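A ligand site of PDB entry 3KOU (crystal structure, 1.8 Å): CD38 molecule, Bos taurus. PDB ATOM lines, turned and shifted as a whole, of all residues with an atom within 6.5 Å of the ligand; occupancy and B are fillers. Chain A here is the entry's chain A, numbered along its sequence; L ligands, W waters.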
ATOM      1  N   GLN A  84     -10.715   5.601 -28.856  1.00  0.00           N
ATOM      2  CA  GLN A  84     -10.422   5.720 -27.414  1.00  0.00           C
ATOM      3  C   GLN A  84      -9.131   6.495 -27.095  1.00  0.00           C
ATOM      4  O   GLN A  84      -8.100   6.323 -27.762  1.00  0.00           O
ATOM      5  CB  GLN A  84     -10.384   4.329 -26.800  1.00  0.00           C
ATOM      6  CG  GLN A  84     -10.404   4.274 -25.269  1.00  0.00           C
ATOM      7  CD  GLN A  84     -10.743   2.867 -24.770  1.00  0.00           C
ATOM      8  OE1 GLN A  84     -11.357   2.076 -25.492  1.00  0.00           O
ATOM      9  NE2 GLN A  84     -10.376   2.572 -23.548  1.00  0.00           N
ATOM     10  N   VAL A  85      -9.192   7.309 -26.058  1.00  0.00           N
ATOM     11  CA  VAL A  85      -8.066   8.142 -25.641  1.00  0.00           C
ATOM     12  C   VAL A  85      -7.791   7.975 -24.157  1.00  0.00           C
ATOM     13  O   VAL A  85      -8.700   8.133 -23.332  1.00  0.00           O
ATOM     14  CB  VAL A  85      -8.343   9.640 -25.921  1.00  0.00           C
ATOM     15  CG1 VAL A  85      -7.215  10.519 -25.362  1.00  0.00           C
ATOM     16  CG2 VAL A  85      -8.541   9.841 -27.428  1.00  0.00           C
ATOM     17  N   PHE A  86      -6.550   7.634 -23.822  1.00  0.00           N
ATOM     18  CA  PHE A  86      -6.058   7.618 -22.452  1.00  0.00           C
ATOM     19  C   PHE A  86      -5.288   8.911 -22.189  1.00  0.00           C
ATOM     20  O   PHE A  86      -4.859   9.592 -23.133  1.00  0.00           O
ATOM     21  CB  PHE A  86      -5.127   6.401 -22.218  1.00  0.00           C
ATOM     22  CG  PHE A  86      -5.810   5.074 -22.358  1.00  0.00           C
ATOM     23  CD1 PHE A  86      -6.450   4.488 -21.277  1.00  0.00           C
ATOM     24  CD2 PHE A  86      -5.840   4.423 -23.588  1.00  0.00           C
ATOM     25  CE1 PHE A  86      -7.098   3.263 -21.421  1.00  0.00           C
ATOM     26  CE2 PHE A  86      -6.483   3.204 -23.725  1.00  0.00           C
ATOM     27  CZ  PHE A  86      -7.094   2.620 -22.650  1.00  0.00           C
ATOM     28  N   TRP A  87      -5.101   9.259 -20.919  1.00  0.00           N
ATOM     29  CA  TRP A  87      -4.327  10.441 -20.524  1.00  0.00           C
ATOM     30  C   TRP A  87      -3.706  10.222 -19.137  1.00  0.00           C
ATOM     31  O   TRP A  87      -4.196   9.425 -18.349  1.00  0.00           O
ATOM     32  CB  TRP A  87      -5.184  11.706 -20.523  1.00  0.00           C
ATOM     33  CG  TRP A  87      -6.355  11.647 -19.581  1.00  0.00           C
ATOM     34  CD1 TRP A  87      -7.620  11.216 -19.882  1.00  0.00           C
ATOM     35  CD2 TRP A  87      -6.375  12.024 -18.205  1.00  0.00           C
ATOM     36  NE1 TRP A  87      -8.430  11.310 -18.768  1.00  0.00           N
ATOM     37  CE2 TRP A  87      -7.680  11.796 -17.732  1.00  0.00           C
ATOM     38  CE3 TRP A  87      -5.406  12.539 -17.330  1.00  0.00           C
ATOM     39  CZ2 TRP A  87      -8.051  12.063 -16.420  1.00  0.00           C
ATOM     40  CZ3 TRP A  87      -5.780  12.796 -16.038  1.00  0.00           C
ATOM     41  CH2 TRP A  87      -7.090  12.569 -15.596  1.00  0.00           C
ATOM     42  N   SER A  88      -2.611  10.932 -18.857  1.00  0.00           N
ATOM     43  CA  SER A  88      -1.996  10.905 -17.525  1.00  0.00           C
ATOM     44  C   SER A  88      -1.225  12.207 -17.336  1.00  0.00           C
ATOM     45  O   SER A  88      -0.333  12.502 -18.132  1.00  0.00           O
ATOM     46  CB  SER A  88      -1.052   9.680 -17.418  1.00  0.00           C
ATOM     47  OG  SER A  88      -0.749   9.355 -16.058  1.00  0.00           O
ATOM     48  N   LYS A  89      -1.621  13.015 -16.340  1.00  0.00           N
ATOM     49  CA  LYS A  89      -0.979  14.295 -16.042  1.00  0.00           C
ATOM     50  C   LYS A  89      -1.262  15.329 -17.126  1.00  0.00           C
ATOM     51  O   LYS A  89      -0.550  16.342 -17.215  1.00  0.00           O
ATOM     52  CB  LYS A  89       0.545  14.163 -15.879  1.00  0.00           C
ATOM     53  CG  LYS A  89       1.039  12.855 -15.271  1.00  0.00           C
ATOM     54  CD  LYS A  89       0.619  12.722 -13.824  1.00  0.00           C
ATOM     55  CE  LYS A  89       1.156  11.409 -13.241  1.00  0.00           C
ATOM     56  NZ  LYS A  89       0.618  11.211 -11.869  1.00  0.00           N
ATOM     57  N   THR A  90      -2.276  15.074 -17.941  1.00  0.00           N
ATOM     58  CA  THR A  90      -2.579  15.927 -19.091  1.00  0.00           C
ATOM     59  C   THR A  90      -4.092  16.154 -19.186  1.00  0.00           C
ATOM     60  O   THR A  90      -4.649  16.302 -20.284  1.00  0.00           O
ATOM     61  CB  THR A  90      -2.101  15.276 -20.387  1.00  0.00           C
ATOM     62  OG1 THR A  90      -2.743  14.001 -20.564  1.00  0.00           O
ATOM     63  CG2 THR A  90      -0.574  15.082 -20.385  1.00  0.00           C
ATOM     64  N   LYS A  91      -4.758  16.206 -18.043  1.00  0.00           N
ATOM     65  CA  LYS A  91      -6.227  16.175 -18.038  1.00  0.00           C
ATOM     66  C   LYS A  91      -6.842  17.213 -18.984  1.00  0.00           C
ATOM     67  O   LYS A  91      -7.595  16.873 -19.883  1.00  0.00           O
ATOM     68  CB  LYS A  91      -6.773  16.363 -16.638  1.00  0.00           C
ATOM     69  CG  LYS A  91      -8.228  15.913 -16.487  1.00  0.00           C
ATOM     70  CD  LYS A  91      -8.685  16.120 -15.054  1.00  0.00           C
ATOM     71  CE  LYS A  91      -8.175  17.440 -14.486  1.00  0.00           C
ATOM     72  NZ  LYS A  91      -8.769  18.627 -15.171  1.00  0.00           N
ATOM     73  N   THR A 105     -12.380  10.031 -24.054  1.00  0.00           N
ATOM     74  CA  THR A 105     -11.674   9.678 -22.821  1.00  0.00           C
ATOM     75  C   THR A 105     -12.624   8.943 -21.888  1.00  0.00           C
ATOM     76  O   THR A 105     -13.829   8.844 -22.180  1.00  0.00           O
ATOM     77  CB  THR A 105     -11.192  10.938 -22.090  1.00  0.00           C
ATOM     78  OG1 THR A 105     -12.344  11.726 -21.690  1.00  0.00           O
ATOM     79  CG2 THR A 105     -10.305  11.761 -23.010  1.00  0.00           C
ATOM     80  N   LEU A 106     -12.105   8.446 -20.779  1.00  0.00           N
ATOM     81  CA  LEU A 106     -12.936   7.776 -19.770  1.00  0.00           C
ATOM     82  C   LEU A 106     -14.061   8.724 -19.350  1.00  0.00           C
ATOM     83  O   LEU A 106     -15.197   8.298 -19.148  1.00  0.00           O
ATOM     84  CB  LEU A 106     -12.071   7.359 -18.576  1.00  0.00           C
ATOM     85  CG  LEU A 106     -12.785   6.554 -17.485  1.00  0.00           C
ATOM     86  CD1 LEU A 106     -13.396   5.233 -18.034  1.00  0.00           C
ATOM     87  CD2 LEU A 106     -11.848   6.290 -16.309  1.00  0.00           C
ATOM     88  N   GLU A 107     -13.738  10.008 -19.275  1.00  0.00           N
ATOM     89  CA  GLU A 107     -14.683  11.020 -18.802  1.00  0.00           C
ATOM     90  C   GLU A 107     -15.807  11.273 -19.825  1.00  0.00           C
ATOM     91  O   GLU A 107     -16.792  11.972 -19.524  1.00  0.00           O
ATOM     92  CB  GLU A 107     -13.938  12.325 -18.406  1.00  0.00           C
ATOM     93  CG  GLU A 107     -13.120  12.220 -17.127  1.00  0.00           C
ATOM     94  CD  GLU A 107     -11.785  11.429 -17.308  1.00  0.00           C
ATOM     95  OE1 GLU A 107     -11.303  11.323 -18.448  1.00  0.00           O
ATOM     96  OE2 GLU A 107     -11.251  10.933 -16.307  1.00  0.00           O
ATOM     97  N   TRP A 150     -12.955   4.741  -9.551  1.00  0.00           N
ATOM     98  CA  TRP A 150     -12.150   5.158 -10.691  1.00  0.00           C
ATOM     99  C   TRP A 150     -11.218   4.020 -11.118  1.00  0.00           C
ATOM    100  O   TRP A 150     -10.990   3.813 -12.302  1.00  0.00           O
ATOM    101  CB  TRP A 150     -11.425   6.492 -10.426  1.00  0.00           C
ATOM    102  CG  TRP A 150     -12.386   7.664 -10.545  1.00  0.00           C
ATOM    103  CD1 TRP A 150     -12.836   8.449  -9.520  1.00  0.00           C
ATOM    104  CD2 TRP A 150     -13.038   8.138 -11.733  1.00  0.00           C
ATOM    105  NE1 TRP A 150     -13.717   9.385 -10.004  1.00  0.00           N
ATOM    106  CE2 TRP A 150     -13.850   9.229 -11.352  1.00  0.00           C
ATOM    107  CE3 TRP A 150     -12.999   7.775 -13.089  1.00  0.00           C
ATOM    108  CZ2 TRP A 150     -14.622   9.943 -12.267  1.00  0.00           C
ATOM    109  CZ3 TRP A 150     -13.757   8.479 -13.986  1.00  0.00           C
ATOM    110  CH2 TRP A 150     -14.571   9.545 -13.579  1.00  0.00           C
ATOM    111  N   SER A 154     -11.644   2.372 -14.777  1.00  0.00           N
ATOM    112  CA  SER A 154     -10.425   2.461 -15.591  1.00  0.00           C
ATOM    113  C   SER A 154      -9.987   1.116 -16.125  1.00  0.00           C
ATOM    114  O   SER A 154      -9.551   1.003 -17.274  1.00  0.00           O
ATOM    115  CB  SER A 154      -9.287   3.101 -14.786  1.00  0.00           C
ATOM    116  OG  SER A 154      -9.570   4.484 -14.507  1.00  0.00           O
ATOM    117  N   PHE A 157     -12.523  -0.033 -18.935  1.00  0.00           N
ATOM    118  CA  PHE A 157     -12.225   0.837 -20.089  1.00  0.00           C
ATOM    119  C   PHE A 157     -11.013   0.311 -20.870  1.00  0.00           C
ATOM    120  O   PHE A 157     -11.047   0.145 -22.114  1.00  0.00           O
ATOM    121  CB  PHE A 157     -11.985   2.241 -19.509  1.00  0.00           C
ATOM    122  CG  PHE A 157     -11.691   3.336 -20.513  1.00  0.00           C
ATOM    123  CD1 PHE A 157     -12.655   3.776 -21.409  1.00  0.00           C
ATOM    124  CD2 PHE A 157     -10.481   4.017 -20.456  1.00  0.00           C
ATOM    125  CE1 PHE A 157     -12.386   4.853 -22.281  1.00  0.00           C
ATOM    126  CE2 PHE A 157     -10.213   5.096 -21.315  1.00  0.00           C
ATOM    127  CZ  PHE A 157     -11.161   5.521 -22.221  1.00  0.00           C
ATOM    128  N   VAL A 167      -2.730   7.756 -26.393  1.00  0.00           N
ATOM    129  CA  VAL A 167      -2.479   8.304 -25.057  1.00  0.00           C
ATOM    130  C   VAL A 167      -1.760   9.662 -25.101  1.00  0.00           C
ATOM    131  O   VAL A 167      -0.803   9.851 -25.878  1.00  0.00           O
ATOM    132  CB  VAL A 167      -1.734   7.317 -24.125  1.00  0.00           C
ATOM    133  CG1 VAL A 167      -0.321   7.079 -24.609  1.00  0.00           C
ATOM    134  CG2 VAL A 167      -1.712   7.865 -22.700  1.00  0.00           C
ATOM    135  N   ASP A 178       4.282   7.462 -15.490  1.00  0.00           N
ATOM    136  CA  ASP A 178       4.335   7.232 -14.048  1.00  0.00           C
ATOM    137  C   ASP A 178       3.769   5.841 -13.767  1.00  0.00           C
ATOM    138  O   ASP A 178       2.559   5.633 -13.892  1.00  0.00           O
ATOM    139  CB  ASP A 178       3.520   8.311 -13.332  1.00  0.00           C
ATOM    140  CG  ASP A 178       3.376   8.076 -11.832  1.00  0.00           C
ATOM    141  OD1 ASP A 178       4.129   7.246 -11.280  1.00  0.00           O
ATOM    142  OD2 ASP A 178       2.504   8.722 -11.213  1.00  0.00           O
ATOM    143  N   MET A 180       3.051   4.360 -11.220  1.00  0.00           N
ATOM    144  CA  MET A 180       2.120   4.286 -10.103  1.00  0.00           C
ATOM    145  C   MET A 180       0.804   4.998 -10.411  1.00  0.00           C
ATOM    146  O   MET A 180      -0.132   4.946  -9.617  1.00  0.00           O
ATOM    147  CB  MET A 180       2.758   4.864  -8.849  1.00  0.00           C
ATOM    148  CG  MET A 180       3.918   4.023  -8.332  1.00  0.00           C
ATOM    149  SD  MET A 180       4.448   4.574  -6.706  1.00  0.00           S
ATOM    150  CE  MET A 180       4.812   6.284  -7.062  1.00  0.00           C
ATOM    151  N   SER A 181       0.737   5.652 -11.572  1.00  0.00           N
ATOM    152  CA  SER A 181      -0.500   6.347 -11.979  1.00  0.00           C
ATOM    153  C   SER A 181      -1.551   5.303 -12.302  1.00  0.00           C
ATOM    154  O   SER A 181      -1.232   4.128 -12.440  1.00  0.00           O
ATOM    155  CB  SER A 181      -0.262   7.234 -13.206  1.00  0.00           C
ATOM    156  OG  SER A 181       0.073   6.453 -14.350  1.00  0.00           O
ATOM    157  N   ILE A 182      -2.800   5.725 -12.444  1.00  0.00           N
ATOM    158  CA  ILE A 182      -3.808   4.805 -12.927  1.00  0.00           C
ATOM    159  C   ILE A 182      -3.479   4.303 -14.346  1.00  0.00           C
ATOM    160  O   ILE A 182      -3.690   3.138 -14.654  1.00  0.00           O
ATOM    161  CB  ILE A 182      -5.201   5.432 -12.869  1.00  0.00           C
ATOM    162  CG1 ILE A 182      -5.600   5.667 -11.408  1.00  0.00           C
ATOM    163  CG2 ILE A 182      -6.245   4.553 -13.595  1.00  0.00           C
ATOM    164  CD1 ILE A 182      -6.930   6.393 -11.257  1.00  0.00           C
ATOM    165  N   PHE A 183      -2.969   5.181 -15.200  1.00  0.00           N
ATOM    166  CA  PHE A 183      -2.588   4.748 -16.535  1.00  0.00           C
ATOM    167  C   PHE A 183      -1.511   3.668 -16.447  1.00  0.00           C
ATOM    168  O   PHE A 183      -1.571   2.659 -17.165  1.00  0.00           O
ATOM    169  CB  PHE A 183      -2.112   5.932 -17.419  1.00  0.00           C
ATOM    170  CG  PHE A 183      -1.607   5.478 -18.782  1.00  0.00           C
ATOM    171  CD1 PHE A 183      -2.493   4.975 -19.724  1.00  0.00           C
ATOM    172  CD2 PHE A 183      -0.260   5.525 -19.091  1.00  0.00           C
ATOM    173  CE1 PHE A 183      -2.054   4.531 -20.958  1.00  0.00           C
ATOM    174  CE2 PHE A 183       0.206   5.046 -20.337  1.00  0.00           C
ATOM    175  CZ  PHE A 183      -0.702   4.582 -21.274  1.00  0.00           C
ATOM    176  N   GLY A 184      -0.544   3.859 -15.564  1.00  0.00           N
ATOM    177  CA  GLY A 184       0.592   2.935 -15.488  1.00  0.00           C
ATOM    178  C   GLY A 184       0.275   1.647 -14.729  1.00  0.00           C
ATOM    179  O   GLY A 184       0.771   0.581 -15.070  1.00  0.00           O
ATOM    180  N   ARG A 185      -0.569   1.751 -13.714  1.00  0.00           N
ATOM    181  CA  ARG A 185      -0.867   0.616 -12.825  1.00  0.00           C
ATOM    182  C   ARG A 185      -2.017  -0.232 -13.306  1.00  0.00           C
ATOM    183  O   ARG A 185      -2.045  -1.429 -13.077  1.00  0.00           O
ATOM    184  CB  ARG A 185      -1.269   1.103 -11.438  1.00  0.00           C
ATOM    185  CG  ARG A 185      -0.147   1.438 -10.506  1.00  0.00           C
ATOM    186  CD  ARG A 185      -0.683   1.656  -9.097  1.00  0.00           C
ATOM    187  NE  ARG A 185      -1.654   2.745  -9.040  1.00  0.00           N
ATOM    188  CZ  ARG A 185      -2.966   2.570  -8.876  1.00  0.00           C
ATOM    189  NH1 ARG A 185      -3.471   1.351  -8.770  1.00  0.00           N
ATOM    190  NH2 ARG A 185      -3.770   3.629  -8.836  1.00  0.00           N
ATOM    191  N   GLU A 187      -4.310   0.727 -16.333  1.00  0.00           N
ATOM    192  CA  GLU A 187      -4.755   0.774 -17.720  1.00  0.00           C
ATOM    193  C   GLU A 187      -3.836   0.058 -18.698  1.00  0.00           C
ATOM    194  O   GLU A 187      -4.273  -0.896 -19.350  1.00  0.00           O
ATOM    195  CB  GLU A 187      -5.071   2.210 -18.165  1.00  0.00           C
ATOM    196  CG  GLU A 187      -6.297   2.723 -17.425  1.00  0.00           C
ATOM    197  CD  GLU A 187      -6.482   4.224 -17.481  1.00  0.00           C
ATOM    198  OE1 GLU A 187      -5.626   4.942 -18.012  1.00  0.00           O
ATOM    199  OE2 GLU A 187      -7.537   4.677 -16.968  1.00  0.00           O
HETATM  200  C1  LIG L   1      -7.879   6.104 -16.471  1.00  0.00           C
HETATM  201  C2  LIG L   1      -8.089   6.903 -17.740  1.00  0.00           C
HETATM  202  F1  LIG L   1      -8.660   6.333 -18.757  1.00  0.00           F
HETATM  203  C3  LIG L   1      -6.817   7.710 -17.906  1.00  0.00           C
HETATM  204  O1  LIG L   1      -6.264   7.490 -19.133  1.00  0.00           O
HETATM  205  O2  LIG L   1      -6.818   6.739 -15.802  1.00  0.00           O
HETATM  206  C4  LIG L   1      -6.024   7.488 -16.613  1.00  0.00           C
HETATM  207  C5  LIG L   1      -5.482   8.698 -15.918  1.00  0.00           C
HETATM  208  O3  LIG L   1      -5.320   8.720 -14.511  1.00  0.00           O
HETATM  209  P1  LIG L   1      -3.864   8.885 -14.023  1.00  0.00           P
HETATM  210  O4  LIG L   1      -3.109   8.163 -15.013  1.00  0.00           O
HETATM  211  O5  LIG L   1      -3.785   8.463 -12.698  1.00  0.00           O
HETATM  212  O6  LIG L   1      -3.575  10.391 -14.257  1.00  0.00           O
HETATM  213  P2  LIG L   1      -3.255  11.505 -13.198  1.00  0.00           P
HETATM  214  O7  LIG L   1      -2.181  11.100 -12.445  1.00  0.00           O
HETATM  215  O8  LIG L   1      -4.446  11.523 -12.390  1.00  0.00           O
HETATM  216  O9  LIG L   1      -3.038  12.727 -13.902  1.00  0.00           O
HETATM  217  O   HOH W   1      -9.236   8.455 -20.654  1.00  0.00           O
HETATM  218  O   HOH W   2      -5.717  12.025  -9.877  1.00  0.00           O
HETATM  219  O   HOH W   3      -2.457   8.945 -10.266  1.00  0.00           O
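Water W1 lies within hydrogen-bond range of the backbone carbonyl oxygen of Val 85, the backbone NH of Leu 106 and an oxygen (O1) of the ligand.
Merely in contact with the ligand: Phe 86 (3.3 Å), Leu 106 (3.6 Å), Ser 154 (3.1 Å), Phe 157 (3.2 Å) and Ser 181 (3.5 Å). Within 4 Å of the ligand: Phe 86, Trp 87, Ser 88, Lys 89, Leu 106, Ser 154, Phe 157, Ser 181, Ile 182, Phe 183 and Glu 187.
O4 of the ligand sits at hydrogen-bond distance from OG of Ser 88. N of Phe 183 is in hydrogen-bond range of O4 of the ligand, 3.0 Å away. OE2 of Glu 187 is covalently linked to C1 of the ligand, 1.5 Å away. An oxygen (O7) of the ligand lies within salt-bridge range of the side-chain amino group of Lys 89. The backbone carbonyl oxygen (O) of Trp 87 sits close to an oxygen (O1) of the ligand (2.9 Å). The backbone NH (N) of Ile 182 sits at hydrogen-bond distance from an oxygen (O5) of the ligand. N of Lys 89 is in hydrogen-bond range of O9 of the ligand (2.8 Å). The backbone NH of Trp 87 is in hydrogen-bond range of an oxygen (O1) of the ligand (2.8 Å).
The side-chain hydroxyl (OG) of Ser 154 sits at hydrogen-bond distance from the side-chain carboxylate (OE2) of Glu 187 (3.2 Å). O of Ile 182 sits at hydrogen-bond distance from N of Glu 187 (3.0 Å). N of Phe 183 sits close to OG of Ser 181. The side-chain hydroxyl (OG) of Ser 181 sits at hydrogen-bond distance from the backbone carbonyl oxygen (O) of Asp 178, at 2.7 Å. The side-chain carboxylate (OE1) of Glu 107 is in hydrogen-bond range of the indole nitrogen (NE1) of Trp 87. The side-chain hydroxyl (OG) of Ser 181 is in hydrogen-bond range of the backbone NH (N) of Gly 184 (2.9 Å). The backbone carbonyl oxygen (O) of Trp 150 is in hydrogen-bond range of the side-chain hydroxyl (OG) of Ser 154 (2.7 Å). The side-chain amino group (NZ) of Lys 89 lies within salt-bridge range of the side-chain carboxylate (OD2) of Asp 178, 3.2 Å away.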
